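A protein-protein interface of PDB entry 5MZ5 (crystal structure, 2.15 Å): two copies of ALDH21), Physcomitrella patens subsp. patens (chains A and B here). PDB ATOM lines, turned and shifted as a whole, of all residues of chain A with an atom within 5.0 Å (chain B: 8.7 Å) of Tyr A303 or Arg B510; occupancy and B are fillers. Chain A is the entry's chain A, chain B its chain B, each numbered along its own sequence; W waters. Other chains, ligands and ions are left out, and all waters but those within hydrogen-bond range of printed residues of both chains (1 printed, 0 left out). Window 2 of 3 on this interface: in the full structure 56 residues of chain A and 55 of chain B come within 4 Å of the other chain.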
ATOM      1  N   VAL A 298      22.576   0.660  28.602  1.00  0.00           N
ATOM      2  CA  VAL A 298      21.324  -0.104  28.621  1.00  0.00           C
ATOM      3  C   VAL A 298      21.519  -1.541  29.153  1.00  0.00           C
ATOM      4  O   VAL A 298      22.185  -2.326  28.485  1.00  0.00           O
ATOM      5  CB  VAL A 298      20.573  -0.093  27.245  1.00  0.00           C
ATOM      6  CG1 VAL A 298      19.166  -0.688  27.386  1.00  0.00           C
ATOM      7  CG2 VAL A 298      20.505   1.314  26.637  1.00  0.00           C
ATOM      8  N   PRO A 299      20.889  -1.942  30.292  1.00  0.00           N
ATOM      9  CA  PRO A 299      20.074  -1.120  31.223  1.00  0.00           C
ATOM     10  C   PRO A 299      20.922  -0.194  32.103  1.00  0.00           C
ATOM     11  O   PRO A 299      20.410   0.794  32.636  1.00  0.00           O
ATOM     12  CB  PRO A 299      19.329  -2.174  32.060  1.00  0.00           C
ATOM     13  CG  PRO A 299      20.261  -3.368  32.087  1.00  0.00           C
ATOM     14  CD  PRO A 299      21.025  -3.339  30.771  1.00  0.00           C
ATOM     15  N   ASP A 300      22.222  -0.509  32.253  1.00  0.00           N
ATOM     16  CA  ASP A 300      23.153   0.274  33.067  1.00  0.00           C
ATOM     17  C   ASP A 300      24.580   0.160  32.535  1.00  0.00           C
ATOM     18  O   ASP A 300      24.825  -0.606  31.594  1.00  0.00           O
ATOM     19  CB  ASP A 300      23.059  -0.117  34.566  1.00  0.00           C
ATOM     20  CG  ASP A 300      23.230  -1.603  34.874  1.00  0.00           C
ATOM     21  OD1 ASP A 300      24.173  -2.224  34.332  1.00  0.00           O
ATOM     22  OD2 ASP A 300      22.452  -2.134  35.698  1.00  0.00           O
ATOM     23  N   LEU A 301      25.516   0.933  33.130  1.00  0.00           N
ATOM     24  CA  LEU A 301      26.928   0.973  32.747  1.00  0.00           C
ATOM     25  C   LEU A 301      27.614  -0.386  32.866  1.00  0.00           C
ATOM     26  O   LEU A 301      28.291  -0.796  31.927  1.00  0.00           O
ATOM     27  CB  LEU A 301      27.690   2.056  33.523  1.00  0.00           C
ATOM     28  CG  LEU A 301      29.206   2.214  33.227  1.00  0.00           C
ATOM     29  CD1 LEU A 301      29.469   2.615  31.775  1.00  0.00           C
ATOM     30  CD2 LEU A 301      29.842   3.219  34.177  1.00  0.00           C
ATOM     31  N   ASP A 302      27.423  -1.079  34.002  1.00  0.00           N
ATOM     32  CA  ASP A 302      28.015  -2.392  34.279  1.00  0.00           C
ATOM     33  C   ASP A 302      27.693  -3.396  33.183  1.00  0.00           C
ATOM     34  O   ASP A 302      28.608  -4.027  32.656  1.00  0.00           O
ATOM     35  CB  ASP A 302      27.535  -2.925  35.642  1.00  0.00           C
ATOM     36  CG  ASP A 302      28.605  -2.935  36.694  1.00  0.00           C
ATOM     37  OD1 ASP A 302      28.888  -1.856  37.262  1.00  0.00           O
ATOM     38  OD2 ASP A 302      29.141  -4.027  36.978  1.00  0.00           O
ATOM     39  N   TYR A 303      26.392  -3.521  32.830  1.00  0.00           N
ATOM     40  CA  TYR A 303      25.943  -4.422  31.785  1.00  0.00           C
ATOM     41  C   TYR A 303      26.470  -3.994  30.411  1.00  0.00           C
ATOM     42  O   TYR A 303      26.871  -4.857  29.642  1.00  0.00           O
ATOM     43  CB  TYR A 303      24.411  -4.572  31.770  1.00  0.00           C
ATOM     44  CG  TYR A 303      23.958  -5.671  30.840  1.00  0.00           C
ATOM     45  CD1 TYR A 303      23.986  -7.006  31.241  1.00  0.00           C
ATOM     46  CD2 TYR A 303      23.571  -5.391  29.533  1.00  0.00           C
ATOM     47  CE1 TYR A 303      23.611  -8.031  30.372  1.00  0.00           C
ATOM     48  CE2 TYR A 303      23.164  -6.404  28.667  1.00  0.00           C
ATOM     49  CZ  TYR A 303      23.197  -7.725  29.088  1.00  0.00           C
ATOM     50  OH  TYR A 303      22.849  -8.745  28.240  1.00  0.00           O
ATOM     51  N   THR A 304      26.487  -2.675  30.118  1.00  0.00           N
ATOM     52  CA  THR A 304      27.010  -2.133  28.849  1.00  0.00           C
ATOM     53  C   THR A 304      28.484  -2.507  28.664  1.00  0.00           C
ATOM     54  O   THR A 304      28.824  -3.056  27.617  1.00  0.00           O
ATOM     55  CB  THR A 304      26.742  -0.625  28.723  1.00  0.00           C
ATOM     56  OG1 THR A 304      25.351  -0.411  28.914  1.00  0.00           O
ATOM     57  CG2 THR A 304      27.170  -0.057  27.362  1.00  0.00           C
ATOM     58  N   ILE A 305      29.324  -2.283  29.706  1.00  0.00           N
ATOM     59  CA  ILE A 305      30.764  -2.603  29.707  1.00  0.00           C
ATOM     60  C   ILE A 305      30.975  -4.101  29.471  1.00  0.00           C
ATOM     61  O   ILE A 305      31.772  -4.460  28.610  1.00  0.00           O
ATOM     62  CB  ILE A 305      31.504  -2.066  30.983  1.00  0.00           C
ATOM     63  CG1 ILE A 305      31.486  -0.515  31.074  1.00  0.00           C
ATOM     64  CG2 ILE A 305      32.949  -2.618  31.136  1.00  0.00           C
ATOM     65  CD1 ILE A 305      32.118   0.315  29.869  1.00  0.00           C
ATOM     66  N   GLN A 306      30.228  -4.964  30.199  1.00  0.00           N
ATOM     67  CA  GLN A 306      30.323  -6.423  30.054  1.00  0.00           C
ATOM     68  C   GLN A 306      30.059  -6.868  28.625  1.00  0.00           C
ATOM     69  O   GLN A 306      30.768  -7.733  28.125  1.00  0.00           O
ATOM     70  CB  GLN A 306      29.351  -7.142  31.005  1.00  0.00           C
ATOM     71  CG  GLN A 306      29.796  -7.158  32.471  1.00  0.00           C
ATOM     72  CD  GLN A 306      28.687  -7.495  33.456  1.00  0.00           C
ATOM     73  OE1 GLN A 306      27.576  -7.922  33.102  1.00  0.00           O
ATOM     74  NE2 GLN A 306      28.978  -7.318  34.741  1.00  0.00           N
ATOM     75  N   ARG A 307      29.043  -6.268  27.959  1.00  0.00           N
ATOM     76  CA  ARG A 307      28.693  -6.623  26.577  1.00  0.00           C
ATOM     77  C   ARG A 307      29.708  -6.093  25.588  1.00  0.00           C
ATOM     78  O   ARG A 307      29.994  -6.761  24.596  1.00  0.00           O
ATOM     79  CB  ARG A 307      27.257  -6.192  26.233  1.00  0.00           C
ATOM     80  CG  ARG A 307      26.204  -6.847  27.145  1.00  0.00           C
ATOM     81  CD  ARG A 307      25.762  -8.207  26.669  1.00  0.00           C
ATOM     82  NE  ARG A 307      26.695  -9.270  27.025  1.00  0.00           N
ATOM     83  CZ  ARG A 307      26.846 -10.398  26.335  1.00  0.00           C
ATOM     84  NH1 ARG A 307      26.141 -10.607  25.224  1.00  0.00           N
ATOM     85  NH2 ARG A 307      27.708 -11.321  26.743  1.00  0.00           N
ATOM     86  N   LEU A 468      20.768  -4.372  18.680  1.00  0.00           N
ATOM     87  CA  LEU A 468      20.200  -3.343  19.520  1.00  0.00           C
ATOM     88  C   LEU A 468      20.353  -3.693  21.005  1.00  0.00           C
ATOM     89  O   LEU A 468      19.814  -4.700  21.477  1.00  0.00           O
ATOM     90  CB  LEU A 468      18.718  -3.102  19.121  1.00  0.00           C
ATOM     91  CG  LEU A 468      17.926  -2.006  19.873  1.00  0.00           C
ATOM     92  CD1 LEU A 468      18.681  -0.629  19.897  1.00  0.00           C
ATOM     93  CD2 LEU A 468      16.534  -1.853  19.260  1.00  0.00           C
ATOM     94  N   ASN A 469      21.116  -2.855  21.714  1.00  0.00           N
ATOM     95  CA  ASN A 469      21.429  -2.932  23.153  1.00  0.00           C
ATOM     96  C   ASN A 469      22.224  -4.203  23.515  1.00  0.00           C
ATOM     97  O   ASN A 469      22.019  -4.861  24.536  1.00  0.00           O
ATOM     98  CB  ASN A 469      20.180  -2.707  24.014  1.00  0.00           C
ATOM     99  CG  ASN A 469      19.694  -1.297  23.808  1.00  0.00           C
ATOM    100  OD1 ASN A 469      20.483  -0.403  23.517  1.00  0.00           O
ATOM    101  ND2 ASN A 469      18.392  -1.072  23.851  1.00  0.00           N
ATOM    102  N   ASP A 470      23.176  -4.496  22.644  1.00  0.00           N
ATOM    103  CA  ASP A 470      24.215  -5.507  22.747  1.00  0.00           C
ATOM    104  C   ASP A 470      25.234  -5.133  21.669  1.00  0.00           C
ATOM    105  O   ASP A 470      24.941  -4.306  20.790  1.00  0.00           O
ATOM    106  CB  ASP A 470      23.694  -6.964  22.618  1.00  0.00           C
ATOM    107  CG  ASP A 470      24.592  -8.030  23.253  1.00  0.00           C
ATOM    108  OD1 ASP A 470      25.809  -7.775  23.415  1.00  0.00           O
ATOM    109  OD2 ASP A 470      24.083  -9.114  23.580  1.00  0.00           O
ATOM    110  N   LEU A 474      26.932 -10.534  18.671  1.00  0.00           N
ATOM    111  CA  LEU A 474      25.796 -11.406  18.922  1.00  0.00           C
ATOM    112  C   LEU A 474      25.275 -12.116  17.672  1.00  0.00           C
ATOM    113  O   LEU A 474      25.003 -11.487  16.655  1.00  0.00           O
ATOM    114  CB  LEU A 474      24.673 -10.635  19.640  1.00  0.00           C
ATOM    115  CG  LEU A 474      23.410 -11.414  20.054  1.00  0.00           C
ATOM    116  CD1 LEU A 474      23.732 -12.512  21.074  1.00  0.00           C
ATOM    117  CD2 LEU A 474      22.369 -10.460  20.629  1.00  0.00           C
ATOM    118  N   LEU B 161      13.680 -14.879  18.992  1.00  0.00           N
ATOM    119  CA  LEU B 161      15.068 -15.310  18.882  1.00  0.00           C
ATOM    120  C   LEU B 161      15.526 -16.067  20.132  1.00  0.00           C
ATOM    121  O   LEU B 161      16.635 -16.595  20.170  1.00  0.00           O
ATOM    122  CB  LEU B 161      15.995 -14.148  18.491  1.00  0.00           C
ATOM    123  CG  LEU B 161      15.954 -13.726  17.006  1.00  0.00           C
ATOM    124  CD1 LEU B 161      16.801 -12.495  16.775  1.00  0.00           C
ATOM    125  CD2 LEU B 161      16.430 -14.875  16.054  1.00  0.00           C
ATOM    126  N   ALA B 165      17.938 -21.224  26.117  1.00  0.00           N
ATOM    127  CA  ALA B 165      18.186 -20.443  27.347  1.00  0.00           C
ATOM    128  C   ALA B 165      19.256 -19.364  27.205  1.00  0.00           C
ATOM    129  O   ALA B 165      19.089 -18.277  27.753  1.00  0.00           O
ATOM    130  CB  ALA B 165      18.514 -21.375  28.516  1.00  0.00           C
ATOM    131  N   ARG B 166      20.338 -19.647  26.467  1.00  0.00           N
ATOM    132  CA  ARG B 166      21.420 -18.681  26.218  1.00  0.00           C
ATOM    133  C   ARG B 166      20.930 -17.464  25.410  1.00  0.00           C
ATOM    134  O   ARG B 166      21.523 -16.387  25.497  1.00  0.00           O
ATOM    135  CB  ARG B 166      22.661 -19.351  25.560  1.00  0.00           C
ATOM    136  CG  ARG B 166      22.356 -20.215  24.327  1.00  0.00           C
ATOM    137  CD  ARG B 166      23.562 -20.459  23.429  1.00  0.00           C
ATOM    138  NE  ARG B 166      23.444 -19.601  22.252  1.00  0.00           N
ATOM    139  CZ  ARG B 166      24.274 -18.613  21.929  1.00  0.00           C
ATOM    140  NH1 ARG B 166      25.361 -18.382  22.658  1.00  0.00           N
ATOM    141  NH2 ARG B 166      24.043 -17.873  20.854  1.00  0.00           N
ATOM    142  N   ASN B 167      19.811 -17.631  24.667  1.00  0.00           N
ATOM    143  CA  ASN B 167      19.202 -16.597  23.834  1.00  0.00           C
ATOM    144  C   ASN B 167      17.998 -15.907  24.473  1.00  0.00           C
ATOM    145  O   ASN B 167      17.253 -15.234  23.779  1.00  0.00           O
ATOM    146  CB  ASN B 167      18.852 -17.171  22.471  1.00  0.00           C
ATOM    147  CG  ASN B 167      20.050 -17.705  21.735  1.00  0.00           C
ATOM    148  OD1 ASN B 167      21.047 -17.008  21.527  1.00  0.00           O
ATOM    149  ND2 ASN B 167      19.981 -18.960  21.347  1.00  0.00           N
ATOM    150  N   LYS B 168      17.841 -16.030  25.799  1.00  0.00           N
ATOM    151  CA  LYS B 168      16.780 -15.406  26.589  1.00  0.00           C
ATOM    152  C   LYS B 168      16.728 -13.877  26.350  1.00  0.00           C
ATOM    153  O   LYS B 168      17.774 -13.232  26.336  1.00  0.00           O
ATOM    154  CB  LYS B 168      17.031 -15.687  28.088  1.00  0.00           C
ATOM    155  CG  LYS B 168      15.965 -15.155  29.026  1.00  0.00           C
ATOM    156  CD  LYS B 168      16.366 -15.309  30.481  1.00  0.00           C
ATOM    157  CE  LYS B 168      15.272 -14.824  31.403  1.00  0.00           C
ATOM    158  NZ  LYS B 168      15.600 -15.070  32.833  1.00  0.00           N
ATOM    159  N   GLY B 169      15.516 -13.335  26.192  1.00  0.00           N
ATOM    160  CA  GLY B 169      15.261 -11.908  26.025  1.00  0.00           C
ATOM    161  C   GLY B 169      15.582 -11.362  24.647  1.00  0.00           C
ATOM    162  O   GLY B 169      15.669 -10.143  24.477  1.00  0.00           O
ATOM    163  N   LEU B 170      15.743 -12.261  23.647  1.00  0.00           N
ATOM    164  CA  LEU B 170      16.070 -11.884  22.276  1.00  0.00           C
ATOM    165  C   LEU B 170      14.901 -12.032  21.330  1.00  0.00           C
ATOM    166  O   LEU B 170      14.148 -13.014  21.381  1.00  0.00           O
ATOM    167  CB  LEU B 170      17.303 -12.639  21.745  1.00  0.00           C
ATOM    168  CG  LEU B 170      18.638 -12.462  22.540  1.00  0.00           C
ATOM    169  CD1 LEU B 170      19.771 -13.186  21.878  1.00  0.00           C
ATOM    170  CD2 LEU B 170      19.030 -10.975  22.691  1.00  0.00           C
ATOM    171  N   GLN B 171      14.761 -11.054  20.446  1.00  0.00           N
ATOM    172  CA  GLN B 171      13.723 -11.045  19.414  1.00  0.00           C
ATOM    173  C   GLN B 171      14.288 -10.310  18.194  1.00  0.00           C
ATOM    174  O   GLN B 171      15.197  -9.505  18.328  1.00  0.00           O
ATOM    175  CB  GLN B 171      12.416 -10.387  19.950  1.00  0.00           C
ATOM    176  CG  GLN B 171      12.525  -8.873  20.200  1.00  0.00           C
ATOM    177  CD  GLN B 171      11.240  -8.254  20.707  1.00  0.00           C
ATOM    178  OE1 GLN B 171      10.176  -8.364  20.096  1.00  0.00           O
ATOM    179  NE2 GLN B 171      11.314  -7.567  21.837  1.00  0.00           N
ATOM    180  N   GLY B 172      13.759 -10.590  17.021  1.00  0.00           N
ATOM    181  CA  GLY B 172      14.230  -9.919  15.821  1.00  0.00           C
ATOM    182  C   GLY B 172      13.155  -9.391  14.902  1.00  0.00           C
ATOM    183  O   GLY B 172      12.045  -9.915  14.866  1.00  0.00           O
ATOM    184  N   LEU B 507      17.199  -6.811  12.789  1.00  0.00           N
ATOM    185  CA  LEU B 507      17.382  -5.988  13.968  1.00  0.00           C
ATOM    186  C   LEU B 507      17.227  -6.960  15.138  1.00  0.00           C
ATOM    187  O   LEU B 507      16.126  -7.435  15.380  1.00  0.00           O
ATOM    188  CB  LEU B 507      16.344  -4.838  14.049  1.00  0.00           C
ATOM    189  CG  LEU B 507      16.493  -3.888  15.253  1.00  0.00           C
ATOM    190  CD1 LEU B 507      17.823  -3.106  15.190  1.00  0.00           C
ATOM    191  CD2 LEU B 507      15.277  -2.966  15.368  1.00  0.00           C
ATOM    192  N   VAL B 508      18.352  -7.353  15.767  1.00  0.00           N
ATOM    193  CA  VAL B 508      18.336  -8.278  16.897  1.00  0.00           C
ATOM    194  C   VAL B 508      18.199  -7.404  18.132  1.00  0.00           C
ATOM    195  O   VAL B 508      19.063  -6.567  18.389  1.00  0.00           O
ATOM    196  CB  VAL B 508      19.560  -9.251  16.956  1.00  0.00           C
ATOM    197  CG1 VAL B 508      19.457 -10.184  18.167  1.00  0.00           C
ATOM    198  CG2 VAL B 508      19.677 -10.073  15.667  1.00  0.00           C
ATOM    199  N   MET B 509      17.091  -7.582  18.869  1.00  0.00           N
ATOM    200  CA  MET B 509      16.725  -6.752  20.006  1.00  0.00           C
ATOM    201  C   MET B 509      16.860  -7.456  21.340  1.00  0.00           C
ATOM    202  O   MET B 509      16.170  -8.440  21.603  1.00  0.00           O
ATOM    203  CB  MET B 509      15.301  -6.221  19.803  1.00  0.00           C
ATOM    204  CG  MET B 509      15.051  -5.675  18.389  1.00  0.00           C
ATOM    205  SD  MET B 509      13.264  -5.543  18.030  1.00  0.00           S
ATOM    206  CE  MET B 509      12.923  -4.028  18.819  1.00  0.00           C
ATOM    207  N   ARG B 510      17.736  -6.924  22.199  1.00  0.00           N
ATOM    208  CA  ARG B 510      18.017  -7.453  23.528  1.00  0.00           C
ATOM    209  C   ARG B 510      17.217  -6.717  24.605  1.00  0.00           C
ATOM    210  O   ARG B 510      17.444  -5.525  24.852  1.00  0.00           O
ATOM    211  CB  ARG B 510      19.535  -7.470  23.783  1.00  0.00           C
ATOM    212  CG  ARG B 510      19.990  -7.329  25.235  1.00  0.00           C
ATOM    213  CD  ARG B 510      20.491  -8.592  25.875  1.00  0.00           C
ATOM    214  NE  ARG B 510      21.484  -9.316  25.076  1.00  0.00           N
ATOM    215  CZ  ARG B 510      21.641 -10.631  25.157  1.00  0.00           C
ATOM    216  NH1 ARG B 510      20.891 -11.344  25.981  1.00  0.00           N
ATOM    217  NH2 ARG B 510      22.532 -11.244  24.400  1.00  0.00           N
ATOM    218  N   ASN B 511      16.260  -7.447  25.223  1.00  0.00           N
ATOM    219  CA  ASN B 511      15.368  -6.973  26.296  1.00  0.00           C
ATOM    220  C   ASN B 511      14.670  -5.638  25.966  1.00  0.00           C
ATOM    221  O   ASN B 511      14.568  -4.754  26.814  1.00  0.00           O
ATOM    222  CB  ASN B 511      16.107  -6.916  27.659  1.00  0.00           C
ATOM    223  CG  ASN B 511      16.621  -8.255  28.129  1.00  0.00           C
ATOM    224  OD1 ASN B 511      15.884  -9.254  28.210  1.00  0.00           O
ATOM    225  ND2 ASN B 511      17.901  -8.298  28.455  1.00  0.00           N
ATOM    226  N   VAL B 512      14.217  -5.489  24.720  1.00  0.00           N
ATOM    227  CA  VAL B 512      13.502  -4.284  24.302  1.00  0.00           C
ATOM    228  C   VAL B 512      12.069  -4.394  24.853  1.00  0.00           C
ATOM    229  O   VAL B 512      11.395  -5.403  24.633  1.00  0.00           O
ATOM    230  CB  VAL B 512      13.591  -4.034  22.764  1.00  0.00           C
ATOM    231  CG1 VAL B 512      12.641  -2.931  22.318  1.00  0.00           C
ATOM    232  CG2 VAL B 512      15.027  -3.690  22.360  1.00  0.00           C
ATOM    233  N   GLY B 513      11.666  -3.390  25.623  1.00  0.00           N
ATOM    234  CA  GLY B 513      10.373  -3.362  26.289  1.00  0.00           C
ATOM    235  C   GLY B 513      10.512  -3.629  27.774  1.00  0.00           C
ATOM    236  O   GLY B 513       9.512  -3.775  28.466  1.00  0.00           O
ATOM    237  N   THR B 514      11.758  -3.726  28.270  1.00  0.00           N
ATOM    238  CA  THR B 514      12.060  -3.894  29.694  1.00  0.00           C
ATOM    239  C   THR B 514      12.299  -2.487  30.232  1.00  0.00           C
ATOM    240  O   THR B 514      13.213  -1.796  29.786  1.00  0.00           O
ATOM    241  CB  THR B 514      13.276  -4.822  29.917  1.00  0.00           C
ATOM    242  OG1 THR B 514      12.953  -6.141  29.472  1.00  0.00           O
ATOM    243  CG2 THR B 514      13.764  -4.848  31.372  1.00  0.00           C
HETATM  244  O   HOH W   1      16.485  -2.247  25.710  1.00  0.00           O
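Arg B510 touches Arg A307.
O of Leu A468 touches CA of Met B509, at 3.99 Å.
CD2 of Leu A468 touches CG2 of Val B512, 3.9 Å away.
Asn A469 touches Arg B510 (O to CG, 3.3 Å).
Leu A474 touches Leu B170 (CD2 to CD2, 3.96 Å).
Val B508 touches Leu A474 (CG1 to CD2, 3.8 Å).
NH2 of Arg B510 touches CD1 of Leu A474 (3.8 Å).
Water W1 lies within hydrogen-bond range of ND2 of Asn A469 and O of Asn B511.
Tyr A303 touches one residue of chain B.
Printed residues of chain A within 4 Å of Arg B510: Tyr A303, Arg A307, Leu A468, Asn A469, Asp A470 and Leu A474.
Of the printed residues of chain A, Leu B170 touches Leu A474 (3.96 Å).
Printed residues of chain B within 4 Å of Asp A470: Arg B510.
Of the printed residues of chain A, Val B512 touches Leu A468 (3.9 Å).
Of the printed residues of chain B, Arg A307 touches Arg B510.
Gln A306 touches none of the printed residues of chain B.
Gln B171 touches none of the printed residues of chain A.
The nearest residue of chain B that does not touch Tyr A303 is Asn B511 (5.0 Å).
The nearest printed residue of chain A that does not touch Met B509 is Asn A469 (6.1 Å).
N of Tyr A303 sits at hydrogen-bond distance from OD1 of Asp A300, at 3.0 Å.
The guanidinium group of Arg A307 lies within salt-bridge range of the side-chain carboxylate of Asp A470, at 3.0 Å.
The backbone carbonyl oxygen (O) of Leu B170 lies within hydrogen-bond range of the backbone NH (N) of Leu B161, 3.1 Å away.
N of Met B509 is in hydrogen-bond range of O of Gln B171 (2.8 Å).
No position is printed for both chains.
Of the 11 pairs that touch across the chains among the printed residues, none has its exchanged pair printed and touching as well.
Of the 14 printed residues of chain A, 6 touch a printed residue of chain B.
Printed residues of chain A that touch a printed residue of chain B: Tyr A303, Arg A307, Leu A468, Asn A469, Asp A470 and Leu A474.
Printed residues of chain B that touch a printed residue of chain A: Leu B170, Val B508, Met B509, Arg B510 and Val B512.
The side-chain hydroxyl (OH) of Tyr A303 lies close to the guanidinium group (NE) of Arg B510 (3.5 Å).
N of Leu A468 sits at hydrogen-bond distance from O of Val B508, 2.8 Å away.
N of Arg B510 lies within hydrogen-bond range of O of Leu A468.
OD2 of Asp A470 lies within salt-bridge range of NH2 of Arg B510 (2.8 Å).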
